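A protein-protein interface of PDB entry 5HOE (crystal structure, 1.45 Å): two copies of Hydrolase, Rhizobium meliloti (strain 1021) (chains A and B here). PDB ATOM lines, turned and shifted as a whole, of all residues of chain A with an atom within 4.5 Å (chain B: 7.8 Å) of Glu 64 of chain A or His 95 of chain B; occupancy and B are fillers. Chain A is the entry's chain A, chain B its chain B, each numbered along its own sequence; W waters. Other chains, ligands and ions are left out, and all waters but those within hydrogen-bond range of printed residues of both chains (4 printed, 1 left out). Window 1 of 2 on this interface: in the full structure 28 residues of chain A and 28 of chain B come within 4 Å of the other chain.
OE1 of Glu 65 of chain B sits at hydrogen-bond distance from OH of Tyr 87 of chain B, 2.9 Å away. The backbone carbonyl oxygen (O) of Met 90 of chain B sits at hydrogen-bond distance from the side-chain hydroxyl (OG) of Ser 94 of chain B, at 2.8 Å. NH2 of Arg 47 of chain A lies within salt-bridge range of OE1 of Glu 64 of chain A (2.9 Å). The side-chain hydroxyl (OG1) of Thr 49 of chain A is in hydrogen-bond range of the side-chain carboxylate (OE2) of Glu 64 of chain A (2.7 Å). N of Glu 65 of chain A lies within hydrogen-bond range of O of Cys 21 of chain A (2.9 Å). The side-chain carboxylate (OE2) of Glu 65 of chain B is in hydrogen-bond range of a ring nitrogen (NE2) of His 95 of chain B (3.2 Å).
Among the printed residues, pairs that only touch across the chains: Glu 64 of chain A with His 95 of chain B (3.1 Å), Arg 41 of chain A with His 95 of chain B (3.6 Å), Glu 65 of chain A with Tyr 87 of chain B (3.7 Å), Arg 41 of chain A with Ser 94 of chain B (3.8 Å) and Arg 41 of chain A with Pro 97 of chain B (3.96 Å).
Glu 64 of chain A touches one residue of chain B. Of the printed residues of chain B, Glu 65 of chain A touches Glu 65 (2.5 Å), Tyr 87 (3.7 Å) and His 95 (3.4 Å). Of the printed residues of chain A, Tyr 87 of chain B touches Glu 65 (3.7 Å). Ala 93 of chain B touches none of the printed residues of chain A. Of chain A, only Arg 41, Glu 64 and Glu 65 come within 4 Å of His 95 of chain B. Of the printed residues of chain A, Leu 96 of chain B touches Arg 41 (3.1 Å). Of the printed residues of chain A, Pro 97 of chain B touches Arg 41 (3.96 Å). Asp 99 of chain B touches none of the printed residues of chain A. The nearest printed residue of chain A that does not touch His 95 of chain B is Gly 66 of chain A (5.1 Å). The nearest printed residue of chain A that does not touch Ser 94 of chain B is Glu 65 of chain A (4.3 Å).
The guanidinium group of Arg 41 of chain A sits at hydrogen-bond distance from the backbone carbonyl oxygen of Leu 96 of chain B (3.1 Å). The backbone NH (N) of Arg 41 of chain A is in hydrogen-bond range of the side-chain hydroxyl (OH) of Tyr 143 of chain B, 3.0 Å away. OE2 of Glu 65 of chain A lies close to OE2 of Glu 65 of chain B (2.5 Å). The backbone carbonyl oxygen of Gly 66 of chain A sits close to the backbone carbonyl oxygen of Ser 94 of chain B (3.2 Å). The side-chain carboxylate (OE1) of Glu 65 of chain A sits at hydrogen-bond distance from a ring nitrogen (NE2) of His 95 of chain B, at 3.4 Å.
Glu 65 of chain A touches its own counterpart, Glu 65 of chain B. Of the 10 pairs that touch across the chains among the printed residues, 1 has its exchanged pair printed and touching as well.
Of the 21 printed residues of chain B, 7 touch a printed residue of chain A.
Water W3 lies within hydrogen-bond range of O of His 95 of chain B (2.7 Å), O of Pro 97 of chain B (2.9 Å), OG of Ser 18 of chain B (3.1 Å) and NH1 of Arg 41 of chain A (3.5 Å). Water W1 lies within hydrogen-bond range of O of Glu 64 of chain A (2.7 Å) and NE2 of His 95 of chain B (3.5 Å). Water W4 lies within hydrogen-bond range of the side-chain hydroxyl (OG) of Ser 94 of chain B and the side-chain carboxylate (OE1) of Glu 65 of chain A. Water W2 lies within hydrogen-bond range of the backbone NH (N) of Gly 66 of chain A, the backbone carbonyl oxygen (O) of Ser 94 of chain B and the guanidinium group (NH2) of Arg 41 of chain A.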
ATOM      1  N   CYS A  21      28.833  -3.072   3.859  1.00  0.00           N
ATOM      2  CA  CYS A  21      29.609  -4.184   3.315  1.00  0.00           C
ATOM      3  C   CYS A  21      28.760  -5.458   3.327  1.00  0.00           C
ATOM      4  O   CYS A  21      28.541  -6.060   4.379  1.00  0.00           O
ATOM      5  CB  CYS A  21      30.887  -4.362   4.118  1.00  0.00           C
ATOM      6  SG  CYS A  21      31.942  -2.882   4.134  1.00  0.00           S
ATOM      7  N   ARG A  41      34.977 -16.620  14.563  1.00  0.00           N
ATOM      8  CA  ARG A  41      35.013 -15.405  13.756  1.00  0.00           C
ATOM      9  C   ARG A  41      36.298 -14.630  14.016  1.00  0.00           C
ATOM     10  O   ARG A  41      36.726 -14.483  15.167  1.00  0.00           O
ATOM     11  CB  ARG A  41      33.823 -14.514  14.125  1.00  0.00           C
ATOM     12  CG  ARG A  41      33.514 -13.403  13.116  1.00  0.00           C
ATOM     13  CD  ARG A  41      32.312 -12.605  13.576  1.00  0.00           C
ATOM     14  NE  ARG A  41      31.918 -11.638  12.567  1.00  0.00           N
ATOM     15  CZ  ARG A  41      30.957 -10.747  12.714  1.00  0.00           C
ATOM     16  NH1 ARG A  41      30.265 -10.698  13.852  1.00  0.00           N
ATOM     17  NH2 ARG A  41      30.682  -9.913  11.706  1.00  0.00           N
ATOM     18  N   TYR A  44      37.400  -7.953  14.620  1.00  0.00           N
ATOM     19  CA  TYR A  44      37.128  -6.907  13.640  1.00  0.00           C
ATOM     20  C   TYR A  44      38.387  -6.447  12.918  1.00  0.00           C
ATOM     21  O   TYR A  44      38.376  -6.277  11.692  1.00  0.00           O
ATOM     22  CB  TYR A  44      36.460  -5.739  14.357  1.00  0.00           C
ATOM     23  CG  TYR A  44      36.055  -4.579  13.488  1.00  0.00           C
ATOM     24  CD1 TYR A  44      35.170  -4.746  12.425  1.00  0.00           C
ATOM     25  CD2 TYR A  44      36.552  -3.314  13.728  1.00  0.00           C
ATOM     26  CE1 TYR A  44      34.786  -3.684  11.640  1.00  0.00           C
ATOM     27  CE2 TYR A  44      36.159  -2.226  12.950  1.00  0.00           C
ATOM     28  CZ  TYR A  44      35.279  -2.423  11.906  1.00  0.00           C
ATOM     29  OH  TYR A  44      34.879  -1.368  11.122  1.00  0.00           O
ATOM     30  N   ARG A  47      39.387  -8.634  10.016  1.00  0.00           N
ATOM     31  CA  ARG A  47      38.430  -8.760   8.930  1.00  0.00           C
ATOM     32  C   ARG A  47      38.765  -7.730   7.860  1.00  0.00           C
ATOM     33  O   ARG A  47      39.369  -6.691   8.146  1.00  0.00           O
ATOM     34  CB  ARG A  47      37.008  -8.524   9.442  1.00  0.00           C
ATOM     35  CG  ARG A  47      36.654  -9.340  10.681  1.00  0.00           C
ATOM     36  CD  ARG A  47      35.186  -9.672  10.813  1.00  0.00           C
ATOM     37  NE  ARG A  47      34.371  -8.660  11.481  1.00  0.00           N
ATOM     38  CZ  ARG A  47      34.028  -8.669  12.769  1.00  0.00           C
ATOM     39  NH1 ARG A  47      34.465  -9.609  13.611  1.00  0.00           N
ATOM     40  NH2 ARG A  47      33.263  -7.695  13.236  1.00  0.00           N
ATOM     41  N   THR A  49      36.700  -5.832   6.425  1.00  0.00           N
ATOM     42  CA  THR A  49      35.909  -4.652   6.743  1.00  0.00           C
ATOM     43  C   THR A  49      36.629  -3.759   7.754  1.00  0.00           C
ATOM     44  O   THR A  49      36.702  -2.532   7.582  1.00  0.00           O
ATOM     45  CB  THR A  49      34.573  -5.125   7.300  1.00  0.00           C
ATOM     46  OG1 THR A  49      34.840  -6.097   8.319  1.00  0.00           O
ATOM     47  CG2 THR A  49      33.691  -5.753   6.187  1.00  0.00           C
ATOM     48  N   ILE A  62      31.508   2.239   8.786  1.00  0.00           N
ATOM     49  CA  ILE A  62      31.414   0.950   8.110  1.00  0.00           C
ATOM     50  C   ILE A  62      30.324   0.133   8.782  1.00  0.00           C
ATOM     51  O   ILE A  62      30.312  -0.012  10.011  1.00  0.00           O
ATOM     52  CB  ILE A  62      32.764   0.208   8.126  1.00  0.00           C
ATOM     53  CG1 ILE A  62      33.618   0.620   6.927  1.00  0.00           C
ATOM     54  CG2 ILE A  62      32.584  -1.316   8.046  1.00  0.00           C
ATOM     55  CD1 ILE A  62      34.019   2.035   6.921  1.00  0.00           C
ATOM     56  N   ILE A  63      29.430  -0.430   7.972  1.00  0.00           N
ATOM     57  CA  ILE A  63      28.344  -1.290   8.429  1.00  0.00           C
ATOM     58  C   ILE A  63      28.596  -2.680   7.859  1.00  0.00           C
ATOM     59  O   ILE A  63      28.771  -2.837   6.643  1.00  0.00           O
ATOM     60  CB  ILE A  63      26.991  -0.752   7.939  1.00  0.00           C
ATOM     61  CG1 ILE A  63      26.753   0.669   8.461  1.00  0.00           C
ATOM     62  CG2 ILE A  63      25.850  -1.670   8.360  1.00  0.00           C
ATOM     63  CD1 ILE A  63      25.905   1.483   7.568  1.00  0.00           C
ATOM     64  N   GLU A  64      28.680  -3.671   8.732  1.00  0.00           N
ATOM     65  CA  GLU A  64      28.948  -5.043   8.323  1.00  0.00           C
ATOM     66  C   GLU A  64      27.642  -5.816   8.192  1.00  0.00           C
ATOM     67  O   GLU A  64      26.841  -5.873   9.141  1.00  0.00           O
ATOM     68  CB  GLU A  64      29.839  -5.722   9.357  1.00  0.00           C
ATOM     69  CG  GLU A  64      31.168  -5.028   9.569  1.00  0.00           C
ATOM     70  CD  GLU A  64      32.023  -5.776  10.556  1.00  0.00           C
ATOM     71  OE1 GLU A  64      31.832  -5.608  11.775  1.00  0.00           O
ATOM     72  OE2 GLU A  64      32.863  -6.560  10.110  1.00  0.00           O
ATOM     73  N   GLU A  65      27.434  -6.416   7.014  1.00  0.00           N
ATOM     74  CA  GLU A  65      26.350  -7.381   6.775  1.00  0.00           C
ATOM     75  C   GLU A  65      26.912  -8.604   6.038  1.00  0.00           C
ATOM     76  O   GLU A  65      26.629  -8.825   4.852  1.00  0.00           O
ATOM     77  CB  GLU A  65      25.190  -6.737   6.004  1.00  0.00           C
ATOM     78  CG  GLU A  65      24.438  -5.647   6.775  1.00  0.00           C
ATOM     79  CD  GLU A  65      23.603  -6.127   7.939  1.00  0.00           C
ATOM     80  OE1 GLU A  65      23.515  -7.338   8.193  1.00  0.00           O
ATOM     81  OE2 GLU A  65      22.998  -5.245   8.603  1.00  0.00           O
ATOM     82  N   GLY A  66      27.690  -9.410   6.759  1.00  0.00           N
ATOM     83  CA  GLY A  66      28.251 -10.639   6.231  1.00  0.00           C
ATOM     84  C   GLY A  66      27.546 -11.840   6.845  1.00  0.00           C
ATOM     85  O   GLY A  66      27.366 -11.915   8.057  1.00  0.00           O
ATOM     86  N   SER B  18      28.922  -7.885  22.580  1.00  0.00           N
ATOM     87  CA  SER B  18      28.203  -7.419  21.396  1.00  0.00           C
ATOM     88  C   SER B  18      26.705  -7.332  21.685  1.00  0.00           C
ATOM     89  O   SER B  18      26.104  -8.287  22.188  1.00  0.00           O
ATOM     90  CB  SER B  18      28.453  -8.352  20.205  1.00  0.00           C
ATOM     91  OG  SER B  18      29.751  -8.160  19.662  1.00  0.00           O
ATOM     92  N   VAL B  19      26.104  -6.191  21.351  1.00  0.00           N
ATOM     93  CA  VAL B  19      24.695  -5.922  21.645  1.00  0.00           C
ATOM     94  C   VAL B  19      23.997  -5.530  20.352  1.00  0.00           C
ATOM     95  O   VAL B  19      24.282  -4.466  19.786  1.00  0.00           O
ATOM     96  CB  VAL B  19      24.530  -4.815  22.696  1.00  0.00           C
ATOM     97  CG1 VAL B  19      23.050  -4.635  23.056  1.00  0.00           C
ATOM     98  CG2 VAL B  19      25.327  -5.124  23.940  1.00  0.00           C
ATOM     99  N   LEU B  20      23.063  -6.361  19.904  1.00  0.00           N
ATOM    100  CA  LEU B  20      22.292  -6.057  18.710  1.00  0.00           C
ATOM    101  C   LEU B  20      20.986  -5.373  19.100  1.00  0.00           C
ATOM    102  O   LEU B  20      20.246  -5.878  19.947  1.00  0.00           O
ATOM    103  CB  LEU B  20      22.013  -7.329  17.901  1.00  0.00           C
ATOM    104  CG  LEU B  20      21.397  -7.131  16.518  1.00  0.00           C
ATOM    105  CD1 LEU B  20      21.840  -8.251  15.562  1.00  0.00           C
ATOM    106  CD2 LEU B  20      19.908  -7.128  16.650  1.00  0.00           C
ATOM    107  N   HIS B  61      30.110  -3.389  22.098  1.00  0.00           N
ATOM    108  CA  HIS B  61      30.049  -3.129  20.669  1.00  0.00           C
ATOM    109  C   HIS B  61      28.580  -3.171  20.286  1.00  0.00           C
ATOM    110  O   HIS B  61      27.926  -4.201  20.464  1.00  0.00           O
ATOM    111  CB  HIS B  61      30.838  -4.198  19.904  1.00  0.00           C
ATOM    112  CG  HIS B  61      30.593  -4.182  18.432  1.00  0.00           C
ATOM    113  ND1 HIS B  61      30.845  -3.074  17.651  1.00  0.00           N
ATOM    114  CD2 HIS B  61      30.089  -5.127  17.599  1.00  0.00           C
ATOM    115  CE1 HIS B  61      30.518  -3.341  16.397  1.00  0.00           C
ATOM    116  NE2 HIS B  61      30.056  -4.580  16.340  1.00  0.00           N
ATOM    117  N   ILE B  63      25.434  -2.981  17.648  1.00  0.00           N
ATOM    118  CA  ILE B  63      25.053  -3.257  16.269  1.00  0.00           C
ATOM    119  C   ILE B  63      23.641  -2.717  16.083  1.00  0.00           C
ATOM    120  O   ILE B  63      22.727  -3.104  16.816  1.00  0.00           O
ATOM    121  CB  ILE B  63      25.090  -4.764  15.976  1.00  0.00           C
ATOM    122  CG1 ILE B  63      26.504  -5.311  16.217  1.00  0.00           C
ATOM    123  CG2 ILE B  63      24.575  -5.061  14.569  1.00  0.00           C
ATOM    124  CD1 ILE B  63      26.541  -6.793  16.543  1.00  0.00           C
ATOM    125  N   GLU B  64      23.455  -1.833  15.111  1.00  0.00           N
ATOM    126  CA  GLU B  64      22.155  -1.223  14.870  1.00  0.00           C
ATOM    127  C   GLU B  64      21.389  -1.970  13.773  1.00  0.00           C
ATOM    128  O   GLU B  64      21.894  -2.128  12.660  1.00  0.00           O
ATOM    129  CB  GLU B  64      22.351   0.242  14.473  1.00  0.00           C
ATOM    130  CG  GLU B  64      22.977   1.110  15.544  1.00  0.00           C
ATOM    131  CD  GLU B  64      23.103   2.559  15.111  1.00  0.00           C
ATOM    132  OE1 GLU B  64      24.025   2.879  14.339  1.00  0.00           O
ATOM    133  OE2 GLU B  64      22.256   3.371  15.528  1.00  0.00           O
ATOM    134  N   GLU B  65      20.139  -2.379  14.078  1.00  0.00           N
ATOM    135  CA  GLU B  65      19.210  -2.948  13.091  1.00  0.00           C
ATOM    136  C   GLU B  65      17.821  -2.331  13.317  1.00  0.00           C
ATOM    137  O   GLU B  65      16.869  -3.004  13.726  1.00  0.00           O
ATOM    138  CB  GLU B  65      19.161  -4.474  13.162  1.00  0.00           C
ATOM    139  CG  GLU B  65      20.489  -5.134  12.754  1.00  0.00           C
ATOM    140  CD  GLU B  65      20.832  -5.085  11.259  1.00  0.00           C
ATOM    141  OE1 GLU B  65      20.037  -4.574  10.461  1.00  0.00           O
ATOM    142  OE2 GLU B  65      21.924  -5.575  10.881  1.00  0.00           O
ATOM    143  N   TYR B  87      13.211 -11.130   9.053  1.00  0.00           N
ATOM    144  CA  TYR B  87      14.594 -10.665   8.925  1.00  0.00           C
ATOM    145  C   TYR B  87      15.473 -11.060  10.104  1.00  0.00           C
ATOM    146  O   TYR B  87      16.679 -11.188   9.931  1.00  0.00           O
ATOM    147  CB  TYR B  87      14.593  -9.125   8.791  1.00  0.00           C
ATOM    148  CG  TYR B  87      15.912  -8.326   8.606  1.00  0.00           C
ATOM    149  CD1 TYR B  87      16.716  -7.946   9.695  1.00  0.00           C
ATOM    150  CD2 TYR B  87      16.274  -7.861   7.352  1.00  0.00           C
ATOM    151  CE1 TYR B  87      17.894  -7.184   9.507  1.00  0.00           C
ATOM    152  CE2 TYR B  87      17.438  -7.087   7.142  1.00  0.00           C
ATOM    153  CZ  TYR B  87      18.244  -6.751   8.221  1.00  0.00           C
ATOM    154  OH  TYR B  87      19.400  -6.014   7.994  1.00  0.00           O
ATOM    155  N   LEU B  88      14.899 -11.232  11.293  1.00  0.00           N
ATOM    156  CA  LEU B  88      15.712 -11.398  12.495  1.00  0.00           C
ATOM    157  C   LEU B  88      16.601 -12.635  12.451  1.00  0.00           C
ATOM    158  O   LEU B  88      17.790 -12.524  12.795  1.00  0.00           O
ATOM    159  CB  LEU B  88      14.835 -11.342  13.756  1.00  0.00           C
ATOM    160  CG  LEU B  88      15.575 -11.432  15.098  1.00  0.00           C
ATOM    161  CD1 LEU B  88      16.543 -10.281  15.282  1.00  0.00           C
ATOM    162  CD2 LEU B  88      14.605 -11.458  16.252  1.00  0.00           C
ATOM    163  N   PRO B  89      16.125 -13.821  12.047  1.00  0.00           N
ATOM    164  CA  PRO B  89      17.058 -14.969  11.997  1.00  0.00           C
ATOM    165  C   PRO B  89      18.291 -14.707  11.146  1.00  0.00           C
ATOM    166  O   PRO B  89      19.400 -15.043  11.575  1.00  0.00           O
ATOM    167  CB  PRO B  89      16.185 -16.118  11.467  1.00  0.00           C
ATOM    168  CG  PRO B  89      14.804 -15.741  11.979  1.00  0.00           C
ATOM    169  CD  PRO B  89      14.739 -14.247  11.762  1.00  0.00           C
ATOM    170  N   MET B  90      18.127 -14.095   9.968  1.00  0.00           N
ATOM    171  CA  MET B  90      19.276 -13.751   9.129  1.00  0.00           C
ATOM    172  C   MET B  90      20.197 -12.758   9.841  1.00  0.00           C
ATOM    173  O   MET B  90      21.426 -12.870   9.783  1.00  0.00           O
ATOM    174  CB  MET B  90      18.779 -13.138   7.809  1.00  0.00           C
ATOM    175  CG  MET B  90      18.124 -14.145   6.856  1.00  0.00           C
ATOM    176  SD  MET B  90      17.547 -13.409   5.292  1.00  0.00           S
ATOM    177  CE  MET B  90      15.878 -12.876   5.625  1.00  0.00           C
ATOM    178  N   ALA B  91      19.620 -11.770  10.503  1.00  0.00           N
ATOM    179  CA  ALA B  91      20.429 -10.773  11.185  1.00  0.00           C
ATOM    180  C   ALA B  91      21.214 -11.395  12.333  1.00  0.00           C
ATOM    181  O   ALA B  91      22.379 -11.049  12.555  1.00  0.00           O
ATOM    182  CB  ALA B  91      19.525  -9.660  11.701  1.00  0.00           C
ATOM    183  N   LEU B  92      20.593 -12.303  13.088  1.00  0.00           N
ATOM    184  CA  LEU B  92      21.294 -12.932  14.198  1.00  0.00           C
ATOM    185  C   LEU B  92      22.509 -13.702  13.692  1.00  0.00           C
ATOM    186  O   LEU B  92      23.618 -13.546  14.211  1.00  0.00           O
ATOM    187  CB  LEU B  92      20.355 -13.884  14.927  1.00  0.00           C
ATOM    188  CG  LEU B  92      19.218 -13.182  15.673  1.00  0.00           C
ATOM    189  CD1 LEU B  92      18.211 -14.212  16.161  1.00  0.00           C
ATOM    190  CD2 LEU B  92      19.715 -12.345  16.833  1.00  0.00           C
ATOM    191  N   ALA B  93      22.322 -14.521  12.654  1.00  0.00           N
ATOM    192  CA  ALA B  93      23.431 -15.338  12.155  1.00  0.00           C
ATOM    193  C   ALA B  93      24.545 -14.477  11.566  1.00  0.00           C
ATOM    194  O   ALA B  93      25.717 -14.880  11.575  1.00  0.00           O
ATOM    195  CB  ALA B  93      22.908 -16.321  11.106  1.00  0.00           C
ATOM    196  N   SER B  94      24.192 -13.311  11.032  1.00  0.00           N
ATOM    197  CA  SER B  94      25.168 -12.378  10.474  1.00  0.00           C
ATOM    198  C   SER B  94      26.030 -11.709  11.537  1.00  0.00           C
ATOM    199  O   SER B  94      27.107 -11.191  11.211  1.00  0.00           O
ATOM    200  CB  SER B  94      24.481 -11.272   9.673  1.00  0.00           C
ATOM    201  OG  SER B  94      23.723 -11.779   8.589  1.00  0.00           O
ATOM    202  N   HIS B  95      25.597 -11.693  12.789  1.00  0.00           N
ATOM    203  CA  HIS B  95      26.275 -10.893  13.796  1.00  0.00           C
ATOM    204  C   HIS B  95      26.767 -11.677  15.000  1.00  0.00           C
ATOM    205  O   HIS B  95      27.327 -11.076  15.925  1.00  0.00           O
ATOM    206  CB  HIS B  95      25.382  -9.735  14.223  1.00  0.00           C
ATOM    207  CG  HIS B  95      25.120  -8.764  13.121  1.00  0.00           C
ATOM    208  ND1 HIS B  95      26.105  -7.958  12.594  1.00  0.00           N
ATOM    209  CD2 HIS B  95      23.996  -8.493  12.419  1.00  0.00           C
ATOM    210  CE1 HIS B  95      25.594  -7.229  11.617  1.00  0.00           C
ATOM    211  NE2 HIS B  95      24.316  -7.534  11.491  1.00  0.00           N
ATOM    212  N   LEU B  96      26.609 -12.996  15.013  1.00  0.00           N
ATOM    213  CA  LEU B  96      27.223 -13.772  16.076  1.00  0.00           C
ATOM    214  C   LEU B  96      28.727 -13.564  16.009  1.00  0.00           C
ATOM    215  O   LEU B  96      29.287 -13.415  14.914  1.00  0.00           O
ATOM    216  CB  LEU B  96      26.909 -15.254  15.959  1.00  0.00           C
ATOM    217  CG  LEU B  96      25.453 -15.639  16.120  1.00  0.00           C
ATOM    218  CD1 LEU B  96      25.385 -17.140  15.981  1.00  0.00           C
ATOM    219  CD2 LEU B  96      24.838 -15.135  17.456  1.00  0.00           C
ATOM    220  N   PRO B  97      29.399 -13.580  17.171  1.00  0.00           N
ATOM    221  CA  PRO B  97      28.880 -13.820  18.520  1.00  0.00           C
ATOM    222  C   PRO B  97      28.131 -12.617  19.083  1.00  0.00           C
ATOM    223  O   PRO B  97      28.549 -11.472  18.887  1.00  0.00           O
ATOM    224  CB  PRO B  97      30.156 -14.065  19.333  1.00  0.00           C
ATOM    225  CG  PRO B  97      31.180 -13.273  18.635  1.00  0.00           C
ATOM    226  CD  PRO B  97      30.862 -13.404  17.174  1.00  0.00           C
ATOM    227  N   LEU B  98      27.040 -12.878  19.791  1.00  0.00           N
ATOM    228  CA  LEU B  98      26.212 -11.839  20.383  1.00  0.00           C
ATOM    229  C   LEU B  98      26.001 -12.191  21.842  1.00  0.00           C
ATOM    230  O   LEU B  98      25.814 -13.362  22.185  1.00  0.00           O
ATOM    231  CB  LEU B  98      24.839 -11.762  19.719  1.00  0.00           C
ATOM    232  CG  LEU B  98      24.755 -11.178  18.317  1.00  0.00           C
ATOM    233  CD1 LEU B  98      23.331 -11.321  17.785  1.00  0.00           C
ATOM    234  CD2 LEU B  98      25.217  -9.752  18.304  1.00  0.00           C
ATOM    235  N   ASP B  99      26.094 -11.190  22.700  1.00  0.00           N
ATOM    236  CA  ASP B  99      25.812 -11.389  24.109  1.00  0.00           C
ATOM    237  C   ASP B  99      24.397 -10.988  24.467  1.00  0.00           C
ATOM    238  O   ASP B  99      23.849 -11.527  25.430  1.00  0.00           O
ATOM    239  CB  ASP B  99      26.830 -10.616  24.942  1.00  0.00           C
ATOM    240  CG  ASP B  99      28.259 -11.141  24.699  1.00  0.00           C
ATOM    241  OD1 ASP B  99      28.628 -12.194  25.275  1.00  0.00           O
ATOM    242  OD2 ASP B  99      28.989 -10.553  23.877  1.00  0.00           O
ATOM    243  N   TYR B 143      28.937 -20.724  18.716  1.00  0.00           N
ATOM    244  CA  TYR B 143      28.571 -19.655  19.630  1.00  0.00           C
ATOM    245  C   TYR B 143      27.201 -19.921  20.263  1.00  0.00           C
ATOM    246  O   TYR B 143      26.297 -20.464  19.612  1.00  0.00           O
ATOM    247  CB  TYR B 143      28.545 -18.321  18.892  1.00  0.00           C
ATOM    248  CG  TYR B 143      29.906 -17.838  18.445  1.00  0.00           C
ATOM    249  CD1 TYR B 143      30.920 -17.599  19.372  1.00  0.00           C
ATOM    250  CD2 TYR B 143      30.189 -17.613  17.089  1.00  0.00           C
ATOM    251  CE1 TYR B 143      32.160 -17.150  18.965  1.00  0.00           C
ATOM    252  CE2 TYR B 143      31.444 -17.164  16.680  1.00  0.00           C
ATOM    253  CZ  TYR B 143      32.418 -16.941  17.616  1.00  0.00           C
ATOM    254  OH  TYR B 143      33.654 -16.487  17.202  1.00  0.00           O
HETATM  255  O   HOH W   1      25.769  -4.378  11.131  1.00  0.00           O
HETATM  256  O   HOH W   2      28.258  -9.081   9.562  1.00  0.00           O
HETATM  257  O   HOH W   3      29.238  -9.482  16.930  1.00  0.00           O
HETATM  258  O   HOH W   4      23.815  -9.769   6.705  1.00  0.00           O
